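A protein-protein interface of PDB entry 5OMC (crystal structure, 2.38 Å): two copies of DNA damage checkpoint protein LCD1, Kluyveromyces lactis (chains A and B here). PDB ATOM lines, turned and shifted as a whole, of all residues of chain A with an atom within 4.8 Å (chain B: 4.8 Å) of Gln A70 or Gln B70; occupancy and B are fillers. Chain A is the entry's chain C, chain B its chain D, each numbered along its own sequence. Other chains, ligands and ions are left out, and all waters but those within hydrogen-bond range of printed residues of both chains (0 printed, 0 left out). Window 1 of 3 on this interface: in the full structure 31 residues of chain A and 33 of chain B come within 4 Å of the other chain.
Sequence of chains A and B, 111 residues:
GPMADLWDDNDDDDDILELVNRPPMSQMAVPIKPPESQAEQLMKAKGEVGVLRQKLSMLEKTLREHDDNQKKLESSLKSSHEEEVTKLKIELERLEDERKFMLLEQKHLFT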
ATOM      1  N   HIS A  66      14.668   0.770 -31.228  1.00  0.00           N
ATOM      2  CA  HIS A  66      13.608   1.753 -30.984  1.00  0.00           C
ATOM      3  C   HIS A  66      12.772   1.296 -29.776  1.00  0.00           C
ATOM      4  O   HIS A  66      12.561   2.100 -28.874  1.00  0.00           O
ATOM      5  CB  HIS A  66      12.717   1.930 -32.238  1.00  0.00           C
ATOM      6  CG  HIS A  66      13.284   2.833 -33.296  1.00  0.00           C
ATOM      7  ND1 HIS A  66      12.483   3.752 -33.960  1.00  0.00           N
ATOM      8  CD2 HIS A  66      14.544   2.925 -33.782  1.00  0.00           C
ATOM      9  CE1 HIS A  66      13.282   4.380 -34.809  1.00  0.00           C
ATOM     10  NE2 HIS A  66      14.529   3.919 -34.738  1.00  0.00           N
ATOM     11  N   ASP A  67      12.383  -0.006 -29.719  1.00  0.00           N
ATOM     12  CA  ASP A  67      11.645  -0.612 -28.601  1.00  0.00           C
ATOM     13  C   ASP A  67      12.396  -0.509 -27.272  1.00  0.00           C
ATOM     14  O   ASP A  67      11.793  -0.101 -26.284  1.00  0.00           O
ATOM     15  CB  ASP A  67      11.232  -2.058 -28.916  1.00  0.00           C
ATOM     16  CG  ASP A  67      10.081  -2.156 -29.911  1.00  0.00           C
ATOM     17  OD1 ASP A  67       9.635  -1.097 -30.416  1.00  0.00           O
ATOM     18  OD2 ASP A  67       9.630  -3.298 -30.194  1.00  0.00           O
ATOM     19  N   ASP A  68      13.704  -0.841 -27.256  1.00  0.00           N
ATOM     20  CA  ASP A  68      14.589  -0.737 -26.084  1.00  0.00           C
ATOM     21  C   ASP A  68      14.709   0.732 -25.622  1.00  0.00           C
ATOM     22  O   ASP A  68      14.743   0.995 -24.413  1.00  0.00           O
ATOM     23  CB  ASP A  68      16.008  -1.289 -26.400  1.00  0.00           C
ATOM     24  CG  ASP A  68      16.087  -2.790 -26.648  1.00  0.00           C
ATOM     25  OD1 ASP A  68      15.187  -3.527 -26.159  1.00  0.00           O
ATOM     26  OD2 ASP A  68      17.064  -3.236 -27.310  1.00  0.00           O
ATOM     27  N   ASN A  69      14.773   1.675 -26.598  1.00  0.00           N
ATOM     28  CA  ASN A  69      14.876   3.113 -26.376  1.00  0.00           C
ATOM     29  C   ASN A  69      13.593   3.672 -25.789  1.00  0.00           C
ATOM     30  O   ASN A  69      13.659   4.507 -24.887  1.00  0.00           O
ATOM     31  CB  ASN A  69      15.199   3.826 -27.679  1.00  0.00           C
ATOM     32  CG  ASN A  69      16.590   4.372 -27.765  1.00  0.00           C
ATOM     33  OD1 ASN A  69      16.874   5.207 -28.620  1.00  0.00           O
ATOM     34  ND2 ASN A  69      17.495   3.923 -26.893  1.00  0.00           N
ATOM     35  N   GLN A  70      12.424   3.213 -26.300  1.00  0.00           N
ATOM     36  CA  GLN A  70      11.095   3.609 -25.809  1.00  0.00           C
ATOM     37  C   GLN A  70      11.042   3.300 -24.323  1.00  0.00           C
ATOM     38  O   GLN A  70      10.714   4.187 -23.540  1.00  0.00           O
ATOM     39  CB  GLN A  70       9.972   2.848 -26.544  1.00  0.00           C
ATOM     40  CG  GLN A  70       8.544   3.317 -26.253  1.00  0.00           C
ATOM     41  CD  GLN A  70       7.855   2.740 -25.023  1.00  0.00           C
ATOM     42  OE1 GLN A  70       7.208   3.463 -24.264  1.00  0.00           O
ATOM     43  NE2 GLN A  70       7.935   1.433 -24.808  1.00  0.00           N
ATOM     44  N   LYS A  71      11.411   2.050 -23.947  1.00  0.00           N
ATOM     45  CA  LYS A  71      11.432   1.514 -22.585  1.00  0.00           C
ATOM     46  C   LYS A  71      12.365   2.312 -21.672  1.00  0.00           C
ATOM     47  O   LYS A  71      11.970   2.646 -20.558  1.00  0.00           O
ATOM     48  CB  LYS A  71      11.783   0.012 -22.586  1.00  0.00           C
ATOM     49  CG  LYS A  71      10.687  -0.871 -23.167  1.00  0.00           C
ATOM     50  CD  LYS A  71      10.811  -2.334 -22.719  1.00  0.00           C
ATOM     51  CE  LYS A  71       9.544  -3.136 -22.980  1.00  0.00           C
ATOM     52  NZ  LYS A  71       9.257  -4.142 -21.911  1.00  0.00           N
ATOM     53  N   LYS A  72      13.571   2.644 -22.161  1.00  0.00           N
ATOM     54  CA  LYS A  72      14.576   3.418 -21.453  1.00  0.00           C
ATOM     55  C   LYS A  72      14.074   4.861 -21.195  1.00  0.00           C
ATOM     56  O   LYS A  72      14.151   5.336 -20.059  1.00  0.00           O
ATOM     57  CB  LYS A  72      15.886   3.430 -22.269  1.00  0.00           C
ATOM     58  CG  LYS A  72      17.112   3.900 -21.499  1.00  0.00           C
ATOM     59  CD  LYS A  72      18.324   4.083 -22.408  1.00  0.00           C
ATOM     60  CE  LYS A  72      18.630   5.532 -22.705  1.00  0.00           C
ATOM     61  NZ  LYS A  72      20.042   5.711 -23.132  1.00  0.00           N
ATOM     62  N   LEU A  73      13.566   5.543 -22.250  1.00  0.00           N
ATOM     63  CA  LEU A  73      13.084   6.933 -22.196  1.00  0.00           C
ATOM     64  C   LEU A  73      11.863   7.100 -21.313  1.00  0.00           C
ATOM     65  O   LEU A  73      11.741   8.131 -20.657  1.00  0.00           O
ATOM     66  CB  LEU A  73      12.802   7.504 -23.593  1.00  0.00           C
ATOM     67  CG  LEU A  73      13.986   7.988 -24.471  1.00  0.00           C
ATOM     68  CD1 LEU A  73      13.473   8.475 -25.777  1.00  0.00           C
ATOM     69  CD2 LEU A  73      14.850   9.100 -23.794  1.00  0.00           C
ATOM     70  N   GLU A  74      10.965   6.092 -21.291  1.00  0.00           N
ATOM     71  CA  GLU A  74       9.764   6.052 -20.448  1.00  0.00           C
ATOM     72  C   GLU A  74      10.165   5.903 -18.970  1.00  0.00           C
ATOM     73  O   GLU A  74       9.589   6.568 -18.116  1.00  0.00           O
ATOM     74  CB  GLU A  74       8.848   4.901 -20.870  1.00  0.00           C
ATOM     75  CG  GLU A  74       7.545   4.829 -20.104  1.00  0.00           C
ATOM     76  CD  GLU A  74       6.544   3.812 -20.612  1.00  0.00           C
ATOM     77  OE1 GLU A  74       5.883   4.091 -21.642  1.00  0.00           O
ATOM     78  OE2 GLU A  74       6.381   2.762 -19.947  1.00  0.00           O
ATOM     79  N   HIS B  66       5.034   1.779 -34.082  1.00  0.00           N
ATOM     80  CA  HIS B  66       5.760   1.767 -32.811  1.00  0.00           C
ATOM     81  C   HIS B  66       6.234   3.210 -32.490  1.00  0.00           C
ATOM     82  O   HIS B  66       6.005   3.688 -31.377  1.00  0.00           O
ATOM     83  CB  HIS B  66       6.952   0.783 -32.875  1.00  0.00           C
ATOM     84  CG  HIS B  66       6.597  -0.665 -32.672  1.00  0.00           C
ATOM     85  ND1 HIS B  66       7.383  -1.496 -31.888  1.00  0.00           N
ATOM     86  CD2 HIS B  66       5.571  -1.393 -33.171  1.00  0.00           C
ATOM     87  CE1 HIS B  66       6.813  -2.690 -31.927  1.00  0.00           C
ATOM     88  NE2 HIS B  66       5.723  -2.684 -32.691  1.00  0.00           N
ATOM     89  N   ASP B  67       6.812   3.921 -33.496  1.00  0.00           N
ATOM     90  CA  ASP B  67       7.259   5.310 -33.369  1.00  0.00           C
ATOM     91  C   ASP B  67       6.108   6.264 -33.017  1.00  0.00           C
ATOM     92  O   ASP B  67       6.269   7.078 -32.113  1.00  0.00           O
ATOM     93  CB  ASP B  67       8.006   5.774 -34.628  1.00  0.00           C
ATOM     94  CG  ASP B  67       9.407   5.217 -34.756  1.00  0.00           C
ATOM     95  OD1 ASP B  67       9.807   4.390 -33.888  1.00  0.00           O
ATOM     96  OD2 ASP B  67      10.111   5.598 -35.728  1.00  0.00           O
ATOM     97  N   ASP B  68       4.943   6.140 -33.709  1.00  0.00           N
ATOM     98  CA  ASP B  68       3.730   6.926 -33.457  1.00  0.00           C
ATOM     99  C   ASP B  68       3.198   6.642 -32.054  1.00  0.00           C
ATOM    100  O   ASP B  68       2.734   7.572 -31.398  1.00  0.00           O
ATOM    101  CB  ASP B  68       2.631   6.606 -34.486  1.00  0.00           C
ATOM    102  CG  ASP B  68       2.909   7.053 -35.910  1.00  0.00           C
ATOM    103  OD1 ASP B  68       3.721   7.996 -36.097  1.00  0.00           O
ATOM    104  OD2 ASP B  68       2.294   6.478 -36.842  1.00  0.00           O
ATOM    105  N   ASN B  69       3.271   5.366 -31.600  1.00  0.00           N
ATOM    106  CA  ASN B  69       2.843   4.895 -30.278  1.00  0.00           C
ATOM    107  C   ASN B  69       3.731   5.466 -29.183  1.00  0.00           C
ATOM    108  O   ASN B  69       3.198   5.877 -28.150  1.00  0.00           O
ATOM    109  CB  ASN B  69       2.867   3.375 -30.209  1.00  0.00           C
ATOM    110  CG  ASN B  69       1.503   2.752 -30.173  1.00  0.00           C
ATOM    111  OD1 ASN B  69       0.771   2.700 -31.184  1.00  0.00           O
ATOM    112  ND2 ASN B  69       1.173   2.213 -29.007  1.00  0.00           N
ATOM    113  N   GLN B  70       5.079   5.495 -29.407  1.00  0.00           N
ATOM    114  CA  GLN B  70       6.038   6.055 -28.461  1.00  0.00           C
ATOM    115  C   GLN B  70       5.638   7.513 -28.180  1.00  0.00           C
ATOM    116  O   GLN B  70       5.484   7.888 -27.017  1.00  0.00           O
ATOM    117  CB  GLN B  70       7.466   5.992 -29.049  1.00  0.00           C
ATOM    118  CG  GLN B  70       8.595   6.488 -28.122  1.00  0.00           C
ATOM    119  CD  GLN B  70       9.934   6.583 -28.819  1.00  0.00           C
ATOM    120  OE1 GLN B  70      10.634   7.602 -28.727  1.00  0.00           O
ATOM    121  NE2 GLN B  70      10.338   5.525 -29.529  1.00  0.00           N
ATOM    122  N   LYS B  71       5.415   8.291 -29.264  1.00  0.00           N
ATOM    123  CA  LYS B  71       5.028   9.697 -29.260  1.00  0.00           C
ATOM    124  C   LYS B  71       3.694   9.925 -28.554  1.00  0.00           C
ATOM    125  O   LYS B  71       3.589  10.854 -27.747  1.00  0.00           O
ATOM    126  CB  LYS B  71       5.019  10.274 -30.691  1.00  0.00           C
ATOM    127  CG  LYS B  71       6.413  10.396 -31.313  1.00  0.00           C
ATOM    128  CD  LYS B  71       6.438  11.365 -32.488  1.00  0.00           C
ATOM    129  CE  LYS B  71       7.850  11.708 -32.905  1.00  0.00           C
ATOM    130  NZ  LYS B  71       7.857  12.651 -34.051  1.00  0.00           N
ATOM    131  N   LYS B  72       2.697   9.070 -28.825  1.00  0.00           N
ATOM    132  CA  LYS B  72       1.367   9.111 -28.225  1.00  0.00           C
ATOM    133  C   LYS B  72       1.440   8.820 -26.716  1.00  0.00           C
ATOM    134  O   LYS B  72       0.854   9.574 -25.941  1.00  0.00           O
ATOM    135  CB  LYS B  72       0.455   8.086 -28.910  1.00  0.00           C
ATOM    136  CG  LYS B  72      -1.040   8.305 -28.693  1.00  0.00           C
ATOM    137  CD  LYS B  72      -1.877   7.157 -29.266  1.00  0.00           C
ATOM    138  CE  LYS B  72      -2.331   7.378 -30.700  1.00  0.00           C
ATOM    139  NZ  LYS B  72      -3.193   6.266 -31.192  1.00  0.00           N
ATOM    140  N   LEU B  73       2.149   7.736 -26.308  1.00  0.00           N
ATOM    141  CA  LEU B  73       2.277   7.300 -24.911  1.00  0.00           C
ATOM    142  C   LEU B  73       3.028   8.307 -24.052  1.00  0.00           C
ATOM    143  O   LEU B  73       2.684   8.468 -22.880  1.00  0.00           O
ATOM    144  CB  LEU B  73       2.949   5.920 -24.818  1.00  0.00           C
ATOM    145  CG  LEU B  73       2.125   4.610 -25.007  1.00  0.00           C
ATOM    146  CD1 LEU B  73       0.993   4.660 -26.100  1.00  0.00           C
ATOM    147  CD2 LEU B  73       3.057   3.448 -25.297  1.00  0.00           C
ATOM    148  N   GLU B  74       4.041   8.980 -24.638  1.00  0.00           N
ATOM    149  CA  GLU B  74       4.831  10.014 -23.983  1.00  0.00           C
ATOM    150  C   GLU B  74       3.969  11.261 -23.753  1.00  0.00           C
ATOM    151  O   GLU B  74       4.049  11.863 -22.686  1.00  0.00           O
ATOM    152  CB  GLU B  74       6.066  10.359 -24.820  1.00  0.00           C
ATOM    153  CG  GLU B  74       7.002  11.353 -24.148  1.00  0.00           C
ATOM    154  CD  GLU B  74       8.304  11.591 -24.886  1.00  0.00           C
ATOM    155  OE1 GLU B  74       9.209  10.731 -24.777  1.00  0.00           O
ATOM    156  OE2 GLU B  74       8.429  12.641 -25.558  1.00  0.00           O
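The side-chain carboxylate of Asp B67 lies within hydrogen-bond range of a ring nitrogen (ND1) of His A66.
The side-chain carboxylate (OD1) of Asp A67 sits at hydrogen-bond distance from a ring nitrogen (ND1) of His B66, 2.7 Å away.
His A66 touches Asp B67, and with the chains exchanged Asp A67 touches His B66.
Gln A70 touches its own counterpart, Gln B70.
Of the 9 printed residues of chain B, 3 touch a printed residue of chain A.
Printed residues of chain B that touch a printed residue of chain A: His B66, Asp B67 and Gln B70.
Hydrophobic or aromatic side chains of chain B that line the printed part of chain A: His B66.
Gln A70 touches one residue of chain B.
Of the printed residues of chain A, Gln B70 touches Gln A70 (3.7 Å).
Printed residues of chain A within 4 Å of His B66: Asp A67 (2.7 Å).
Of the printed residues of chain B, His A66 touches Asp B67.
Of the printed residues of chain A, Asp B67 touches His A66 (2.8 Å).
Printed residues of chain B within 4 Å of Asp A67: His B66.
The nearest residue of chain B that does not touch Gln A70 is Leu B73 (4.3 Å).
The nearest printed residue of chain B that does not touch His A66 is Gln B70 (4.1 Å).
OE1 of Gln A70 sits close to OE1 of Glu A74.
Among the printed residues, pairs that only touch across the chains: Gln A70 with Gln B70.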
